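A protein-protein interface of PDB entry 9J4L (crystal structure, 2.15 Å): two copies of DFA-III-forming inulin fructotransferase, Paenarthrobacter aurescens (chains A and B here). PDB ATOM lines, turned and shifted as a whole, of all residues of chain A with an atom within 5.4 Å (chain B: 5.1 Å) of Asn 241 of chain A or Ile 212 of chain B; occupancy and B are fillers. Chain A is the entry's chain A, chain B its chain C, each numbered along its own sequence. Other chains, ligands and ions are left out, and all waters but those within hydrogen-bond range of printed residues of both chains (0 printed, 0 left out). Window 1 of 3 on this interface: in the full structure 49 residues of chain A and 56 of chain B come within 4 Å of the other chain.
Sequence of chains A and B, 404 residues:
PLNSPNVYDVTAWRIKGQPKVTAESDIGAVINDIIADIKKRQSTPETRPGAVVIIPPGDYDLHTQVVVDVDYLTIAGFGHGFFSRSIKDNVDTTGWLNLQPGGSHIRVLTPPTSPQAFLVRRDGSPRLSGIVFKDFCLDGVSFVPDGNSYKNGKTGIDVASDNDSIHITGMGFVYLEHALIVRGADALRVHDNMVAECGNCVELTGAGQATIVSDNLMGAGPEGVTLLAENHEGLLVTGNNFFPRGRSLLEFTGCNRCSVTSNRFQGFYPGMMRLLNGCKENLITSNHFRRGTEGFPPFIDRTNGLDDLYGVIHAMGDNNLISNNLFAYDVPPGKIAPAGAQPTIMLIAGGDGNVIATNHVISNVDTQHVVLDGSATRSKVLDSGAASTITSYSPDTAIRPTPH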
ATOM      1  N   ASP A 215     -10.291  -8.409 -15.552  1.00  0.00           N
ATOM      2  CA  ASP A 215      -9.723  -9.621 -14.984  1.00  0.00           C
ATOM      3  C   ASP A 215      -8.913 -10.430 -15.987  1.00  0.00           C
ATOM      4  O   ASP A 215      -8.733 -11.633 -15.828  1.00  0.00           O
ATOM      5  CB  ASP A 215     -10.812 -10.466 -14.310  1.00  0.00           C
ATOM      6  CG  ASP A 215     -11.483  -9.725 -13.141  1.00  0.00           C
ATOM      7  OD1 ASP A 215     -10.770  -9.020 -12.382  1.00  0.00           O
ATOM      8  OD2 ASP A 215     -12.726  -9.809 -12.998  1.00  0.00           O
ATOM      9  N   ASN A 216      -8.396  -9.753 -17.008  1.00  0.00           N
ATOM     10  CA  ASN A 216      -7.532 -10.386 -17.991  1.00  0.00           C
ATOM     11  C   ASN A 216      -6.039 -10.332 -17.686  1.00  0.00           C
ATOM     12  O   ASN A 216      -5.533  -9.377 -17.088  1.00  0.00           O
ATOM     13  CB  ASN A 216      -7.756  -9.784 -19.381  1.00  0.00           C
ATOM     14  CG  ASN A 216      -9.186  -9.886 -19.835  1.00  0.00           C
ATOM     15  OD1 ASN A 216      -9.653 -10.971 -20.209  1.00  0.00           O
ATOM     16  ND2 ASN A 216      -9.899  -8.746 -19.819  1.00  0.00           N
ATOM     17  N   LEU A 217      -5.340 -11.340 -18.192  1.00  0.00           N
ATOM     18  CA  LEU A 217      -3.883 -11.349 -18.281  1.00  0.00           C
ATOM     19  C   LEU A 217      -3.494 -11.059 -19.730  1.00  0.00           C
ATOM     20  O   LEU A 217      -3.860 -11.807 -20.635  1.00  0.00           O
ATOM     21  CB  LEU A 217      -3.368 -12.746 -17.911  1.00  0.00           C
ATOM     22  CG  LEU A 217      -3.436 -13.107 -16.435  1.00  0.00           C
ATOM     23  CD1 LEU A 217      -3.182 -14.597 -16.211  1.00  0.00           C
ATOM     24  CD2 LEU A 217      -2.440 -12.242 -15.655  1.00  0.00           C
ATOM     25  N   MET A 218      -2.735  -9.999 -19.964  1.00  0.00           N
ATOM     26  CA  MET A 218      -2.392  -9.651 -21.346  1.00  0.00           C
ATOM     27  C   MET A 218      -0.932  -9.236 -21.549  1.00  0.00           C
ATOM     28  O   MET A 218      -0.379  -8.459 -20.761  1.00  0.00           O
ATOM     29  CB  MET A 218      -3.328  -8.558 -21.865  1.00  0.00           C
ATOM     30  CG  MET A 218      -4.794  -8.954 -21.955  1.00  0.00           C
ATOM     31  SD  MET A 218      -5.702  -7.704 -22.883  1.00  0.00           S
ATOM     32  CE  MET A 218      -7.392  -7.882 -22.300  1.00  0.00           C
ATOM     33  N   GLY A 239      -9.297  -4.385 -13.181  1.00  0.00           N
ATOM     34  CA  GLY A 239      -8.893  -5.697 -12.708  1.00  0.00           C
ATOM     35  C   GLY A 239      -7.968  -6.475 -13.633  1.00  0.00           C
ATOM     36  O   GLY A 239      -7.746  -7.673 -13.417  1.00  0.00           O
ATOM     37  N   ASN A 240      -7.392  -5.803 -14.628  1.00  0.00           N
ATOM     38  CA  ASN A 240      -6.487  -6.461 -15.575  1.00  0.00           C
ATOM     39  C   ASN A 240      -5.038  -6.430 -15.125  1.00  0.00           C
ATOM     40  O   ASN A 240      -4.623  -5.508 -14.416  1.00  0.00           O
ATOM     41  CB  ASN A 240      -6.601  -5.831 -16.975  1.00  0.00           C
ATOM     42  CG  ASN A 240      -8.031  -5.805 -17.485  1.00  0.00           C
ATOM     43  OD1 ASN A 240      -8.567  -6.829 -17.964  1.00  0.00           O
ATOM     44  ND2 ASN A 240      -8.655  -4.629 -17.395  1.00  0.00           N
ATOM     45  N   ASN A 241      -4.261  -7.406 -15.589  1.00  0.00           N
ATOM     46  CA  ASN A 241      -2.821  -7.440 -15.349  1.00  0.00           C
ATOM     47  C   ASN A 241      -2.066  -7.392 -16.674  1.00  0.00           C
ATOM     48  O   ASN A 241      -1.979  -8.390 -17.401  1.00  0.00           O
ATOM     49  CB  ASN A 241      -2.422  -8.693 -14.549  1.00  0.00           C
ATOM     50  CG  ASN A 241      -1.035  -8.577 -13.916  1.00  0.00           C
ATOM     51  OD1 ASN A 241      -0.079  -8.215 -14.580  1.00  0.00           O
ATOM     52  ND2 ASN A 241      -0.912  -9.005 -12.664  1.00  0.00           N
ATOM     53  N   PHE A 242      -1.626  -6.199 -17.001  1.00  0.00           N
ATOM     54  CA  PHE A 242      -1.001  -5.974 -18.271  1.00  0.00           C
ATOM     55  C   PHE A 242       0.498  -6.098 -18.137  1.00  0.00           C
ATOM     56  O   PHE A 242       1.128  -5.347 -17.412  1.00  0.00           O
ATOM     57  CB  PHE A 242      -1.361  -4.601 -18.816  1.00  0.00           C
ATOM     58  CG  PHE A 242      -2.786  -4.427 -19.215  1.00  0.00           C
ATOM     59  CD1 PHE A 242      -3.263  -4.974 -20.383  1.00  0.00           C
ATOM     60  CD2 PHE A 242      -3.631  -3.658 -18.447  1.00  0.00           C
ATOM     61  CE1 PHE A 242      -4.572  -4.791 -20.760  1.00  0.00           C
ATOM     62  CE2 PHE A 242      -4.938  -3.458 -18.820  1.00  0.00           C
ATOM     63  CZ  PHE A 242      -5.413  -4.033 -19.978  1.00  0.00           C
ATOM     64  N   PHE A 243       1.078  -6.957 -18.911  1.00  0.00           N
ATOM     65  CA  PHE A 243       2.496  -7.066 -18.902  1.00  0.00           C
ATOM     66  C   PHE A 243       3.112  -7.126 -20.275  1.00  0.00           C
ATOM     67  O   PHE A 243       2.452  -6.859 -21.254  1.00  0.00           O
ATOM     68  CB  PHE A 243       2.847  -8.380 -18.199  1.00  0.00           C
ATOM     69  CG  PHE A 243       2.013  -9.546 -18.653  1.00  0.00           C
ATOM     70  CD1 PHE A 243       2.307 -10.210 -19.830  1.00  0.00           C
ATOM     71  CD2 PHE A 243       0.924  -9.968 -17.911  1.00  0.00           C
ATOM     72  CE1 PHE A 243       1.536 -11.270 -20.257  1.00  0.00           C
ATOM     73  CE2 PHE A 243       0.148 -11.028 -18.334  1.00  0.00           C
ATOM     74  CZ  PHE A 243       0.455 -11.680 -19.509  1.00  0.00           C
ATOM     75  N   ARG A 264      -3.058  -3.417 -13.112  1.00  0.00           N
ATOM     76  CA  ARG A 264      -1.634  -3.472 -13.044  1.00  0.00           C
ATOM     77  C   ARG A 264      -0.958  -3.412 -14.402  1.00  0.00           C
ATOM     78  O   ARG A 264      -1.267  -4.193 -15.265  1.00  0.00           O
ATOM     79  CB  ARG A 264      -1.222  -4.741 -12.362  1.00  0.00           C
ATOM     80  CG  ARG A 264       0.243  -4.922 -12.105  1.00  0.00           C
ATOM     81  CD  ARG A 264       0.832  -6.045 -12.867  1.00  0.00           C
ATOM     82  NE  ARG A 264       2.273  -6.023 -12.798  1.00  0.00           N
ATOM     83  CZ  ARG A 264       3.061  -6.928 -13.326  1.00  0.00           C
ATOM     84  NH1 ARG A 264       2.563  -7.931 -13.993  1.00  0.00           N
ATOM     85  NH2 ARG A 264       4.343  -6.833 -13.199  1.00  0.00           N
ATOM     86  N   LEU B 188      -0.953 -16.639 -12.745  1.00  0.00           N
ATOM     87  CA  LEU B 188      -2.020 -17.382 -12.039  1.00  0.00           C
ATOM     88  C   LEU B 188      -3.244 -16.488 -11.840  1.00  0.00           C
ATOM     89  O   LEU B 188      -3.096 -15.293 -11.624  1.00  0.00           O
ATOM     90  CB  LEU B 188      -1.493 -17.870 -10.680  1.00  0.00           C
ATOM     91  CG  LEU B 188      -2.525 -18.315  -9.644  1.00  0.00           C
ATOM     92  CD1 LEU B 188      -3.153 -19.646 -10.011  1.00  0.00           C
ATOM     93  CD2 LEU B 188      -1.912 -18.389  -8.257  1.00  0.00           C
ATOM     94  N   ARG B 189      -4.406 -17.073 -11.984  1.00  0.00           N
ATOM     95  CA  ARG B 189      -5.632 -16.390 -11.650  1.00  0.00           C
ATOM     96  C   ARG B 189      -6.404 -17.225 -10.610  1.00  0.00           C
ATOM     97  O   ARG B 189      -6.781 -18.375 -10.866  1.00  0.00           O
ATOM     98  CB  ARG B 189      -6.484 -16.167 -12.908  1.00  0.00           C
ATOM     99  CG  ARG B 189      -5.982 -15.073 -13.845  1.00  0.00           C
ATOM    100  CD  ARG B 189      -6.660 -15.182 -15.220  1.00  0.00           C
ATOM    101  NE  ARG B 189      -6.273 -16.416 -15.906  1.00  0.00           N
ATOM    102  CZ  ARG B 189      -6.920 -17.002 -16.919  1.00  0.00           C
ATOM    103  NH1 ARG B 189      -8.076 -16.539 -17.377  1.00  0.00           N
ATOM    104  NH2 ARG B 189      -6.395 -18.075 -17.487  1.00  0.00           N
ATOM    105  N   VAL B 190      -6.628 -16.639  -9.434  1.00  0.00           N
ATOM    106  CA  VAL B 190      -7.511 -17.233  -8.449  1.00  0.00           C
ATOM    107  C   VAL B 190      -8.743 -16.338  -8.394  1.00  0.00           C
ATOM    108  O   VAL B 190      -8.701 -15.239  -7.832  1.00  0.00           O
ATOM    109  CB  VAL B 190      -6.865 -17.275  -7.050  1.00  0.00           C
ATOM    110  CG1 VAL B 190      -7.832 -17.881  -6.030  1.00  0.00           C
ATOM    111  CG2 VAL B 190      -5.545 -18.058  -7.063  1.00  0.00           C
ATOM    112  N   ALA B 210       2.959 -11.632 -12.057  1.00  0.00           N
ATOM    113  CA  ALA B 210       1.871 -11.464 -13.020  1.00  0.00           C
ATOM    114  C   ALA B 210       0.599 -12.196 -12.606  1.00  0.00           C
ATOM    115  O   ALA B 210      -0.034 -12.876 -13.411  1.00  0.00           O
ATOM    116  CB  ALA B 210       2.316 -11.914 -14.409  1.00  0.00           C
ATOM    117  N   THR B 211       0.278 -12.161 -11.321  1.00  0.00           N
ATOM    118  CA  THR B 211      -0.846 -12.937 -10.806  1.00  0.00           C
ATOM    119  C   THR B 211      -2.025 -12.032 -10.440  1.00  0.00           C
ATOM    120  O   THR B 211      -1.839 -10.829 -10.214  1.00  0.00           O
ATOM    121  CB  THR B 211      -0.396 -13.870  -9.659  1.00  0.00           C
ATOM    122  OG1 THR B 211       0.433 -14.919 -10.208  1.00  0.00           O
ATOM    123  CG2 THR B 211      -1.600 -14.490  -8.914  1.00  0.00           C
ATOM    124  N   ILE B 212      -3.239 -12.558 -10.598  1.00  0.00           N
ATOM    125  CA  ILE B 212      -4.461 -11.855 -10.198  1.00  0.00           C
ATOM    126  C   ILE B 212      -5.247 -12.691  -9.194  1.00  0.00           C
ATOM    127  O   ILE B 212      -5.495 -13.892  -9.418  1.00  0.00           O
ATOM    128  CB  ILE B 212      -5.401 -11.533 -11.388  1.00  0.00           C
ATOM    129  CG1 ILE B 212      -4.633 -10.879 -12.542  1.00  0.00           C
ATOM    130  CG2 ILE B 212      -6.566 -10.627 -10.931  1.00  0.00           C
ATOM    131  CD1 ILE B 212      -5.510 -10.538 -13.741  1.00  0.00           C
ATOM    132  N   VAL B 213      -5.597 -12.069  -8.074  1.00  0.00           N
ATOM    133  CA  VAL B 213      -6.533 -12.677  -7.126  1.00  0.00           C
ATOM    134  C   VAL B 213      -7.762 -11.779  -7.048  1.00  0.00           C
ATOM    135  O   VAL B 213      -7.673 -10.657  -6.583  1.00  0.00           O
ATOM    136  CB  VAL B 213      -5.908 -12.861  -5.723  1.00  0.00           C
ATOM    137  CG1 VAL B 213      -6.933 -13.435  -4.735  1.00  0.00           C
ATOM    138  CG2 VAL B 213      -4.669 -13.761  -5.799  1.00  0.00           C
ATOM    139  N   SER B 214      -8.876 -12.230  -7.617  1.00  0.00           N
ATOM    140  CA  SER B 214     -10.025 -11.347  -7.787  1.00  0.00           C
ATOM    141  C   SER B 214     -11.386 -12.005  -7.501  1.00  0.00           C
ATOM    142  O   SER B 214     -11.595 -13.209  -7.765  1.00  0.00           O
ATOM    143  CB  SER B 214     -10.009 -10.678  -9.164  1.00  0.00           C
ATOM    144  OG  SER B 214     -10.242 -11.642 -10.184  1.00  0.00           O
ATOM    145  N   GLY B 234       4.312  -7.768  -8.998  1.00  0.00           N
ATOM    146  CA  GLY B 234       3.200  -7.467  -9.904  1.00  0.00           C
ATOM    147  C   GLY B 234       1.939  -8.300  -9.653  1.00  0.00           C
ATOM    148  O   GLY B 234       1.189  -8.608 -10.597  1.00  0.00           O
ATOM    149  N   LEU B 235       1.727  -8.702  -8.393  1.00  0.00           N
ATOM    150  CA  LEU B 235       0.458  -9.309  -7.979  1.00  0.00           C
ATOM    151  C   LEU B 235      -0.673  -8.263  -7.877  1.00  0.00           C
ATOM    152  O   LEU B 235      -0.493  -7.201  -7.297  1.00  0.00           O
ATOM    153  CB  LEU B 235       0.638 -10.036  -6.650  1.00  0.00           C
ATOM    154  CG  LEU B 235      -0.585 -10.569  -5.901  1.00  0.00           C
ATOM    155  CD1 LEU B 235      -1.300 -11.641  -6.707  1.00  0.00           C
ATOM    156  CD2 LEU B 235      -0.180 -11.113  -4.538  1.00  0.00           C
ATOM    157  N   LEU B 236      -1.816  -8.549  -8.494  1.00  0.00           N
ATOM    158  CA  LEU B 236      -2.982  -7.665  -8.420  1.00  0.00           C
ATOM    159  C   LEU B 236      -4.083  -8.319  -7.571  1.00  0.00           C
ATOM    160  O   LEU B 236      -4.486  -9.460  -7.826  1.00  0.00           O
ATOM    161  CB  LEU B 236      -3.490  -7.373  -9.827  1.00  0.00           C
ATOM    162  CG  LEU B 236      -4.748  -6.510 -10.029  1.00  0.00           C
ATOM    163  CD1 LEU B 236      -4.601  -5.140  -9.385  1.00  0.00           C
ATOM    164  CD2 LEU B 236      -5.015  -6.354 -11.519  1.00  0.00           C
ATOM    165  N   THR B 238      -7.735  -7.704  -6.158  1.00  0.00           N
ATOM    166  CA  THR B 238      -8.812  -6.754  -6.435  1.00  0.00           C
ATOM    167  C   THR B 238     -10.217  -7.352  -6.444  1.00  0.00           C
ATOM    168  O   THR B 238     -10.410  -8.489  -6.855  1.00  0.00           O
ATOM    169  CB  THR B 238      -8.576  -5.962  -7.734  1.00  0.00           C
ATOM    170  OG1 THR B 238      -9.556  -4.925  -7.825  1.00  0.00           O
ATOM    171  CG2 THR B 238      -8.708  -6.874  -8.943  1.00  0.00           C
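Of the 10 printed residues of chain A, 7 touch a printed residue of chain B.
Hydrophobic or aromatic side chains of chain A that line the printed part of chain B: Leu 217.
Among the printed residues, 17 pairs touch across the chains.
Among the printed residues, merely in contact across the chains: Asp 215 of chain A with Ile 212 of chain B (3.99 Å), Asn 216 of chain A with Ile 212 of chain B (3.5 Å), Leu 217 of chain A with Arg 189 of chain B (3.6 Å), Leu 217 of chain A with Ala 210 of chain B (3.4 Å), Leu 217 of chain A with Ile 212 of chain B (3.999 Å), Gly 239 of chain A with Ile 212 of chain B (3.6 Å), Gly 239 of chain A with Leu 236 of chain B (3.6 Å), Gly 239 of chain A with Thr 238 of chain B (3.9 Å), Asn 240 of chain A with Leu 236 of chain B (3.0 Å), Asn 241 of chain A with Ala 210 of chain B (3.5 Å), Asn 241 of chain A with Ile 212 of chain B (3.7 Å), Arg 264 of chain A with Ala 210 of chain B (3.7 Å), Arg 264 of chain A with Gly 234 of chain B (3.4 Å) and Arg 264 of chain A with Leu 236 of chain B (3.9 Å).
No position is printed for both chains.
Of the 17 pairs that touch across the chains among the printed residues, none has its exchanged pair printed and touching as well.
N of Asp 215 of chain A sits close to O of Gly 239 of chain A, 3.4 Å away.
ND2 of Asn 216 of chain A sits at hydrogen-bond distance from OD1 of Asn 240 of chain A, at 3.0 Å.
The backbone carbonyl oxygen of Asn 216 of chain A is in hydrogen-bond range of the backbone NH of Asn 241 of chain A, at 2.8 Å.
The backbone NH (N) of Met 218 of chain A is in hydrogen-bond range of the backbone carbonyl oxygen (O) of Asn 241 of chain A (3.1 Å).
The backbone NH (N) of Phe 242 of chain A lies within hydrogen-bond range of the backbone carbonyl oxygen (O) of Arg 264 of chain A, 2.7 Å away.
O of Val 213 of chain B lies within hydrogen-bond range of N of Thr 238 of chain B (3.0 Å).
Asn 241 of chain A touches four residues of chain B.
Of the printed residues of chain A, Thr 211 of chain B touches Asn 241 (3.2 Å).
Of the printed residues of chain A, Ile 212 of chain B touches Asp 215, Asn 216, Leu 217, Gly 239 and Asn 241.
Of the printed residues of chain A, Leu 236 of chain B touches Gly 239 (3.6 Å), Asn 240 (3.0 Å) and Arg 264 (3.9 Å).
The nearest printed residue of chain A that does not touch Ile 212 of chain B is Asn 240 of chain A (4.4 Å).
The nearest printed residue of chain A that does not touch Ala 210 of chain B is Phe 243 of chain A (4.2 Å).
OD1 of Asp 215 of chain A is in hydrogen-bond range of OG of Ser 214 of chain B (3.5 Å).
The side-chain amide nitrogen (ND2) of Asn 241 of chain A lies within hydrogen-bond range of the backbone carbonyl oxygen (O) of Thr 211 of chain B, 3.2 Å away.
The backbone carbonyl oxygen (O) of Gly 234 of chain B lies within hydrogen-bond range of the side-chain amide nitrogen (ND2) of Asn 241 of chain A, 3.0 Å away.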
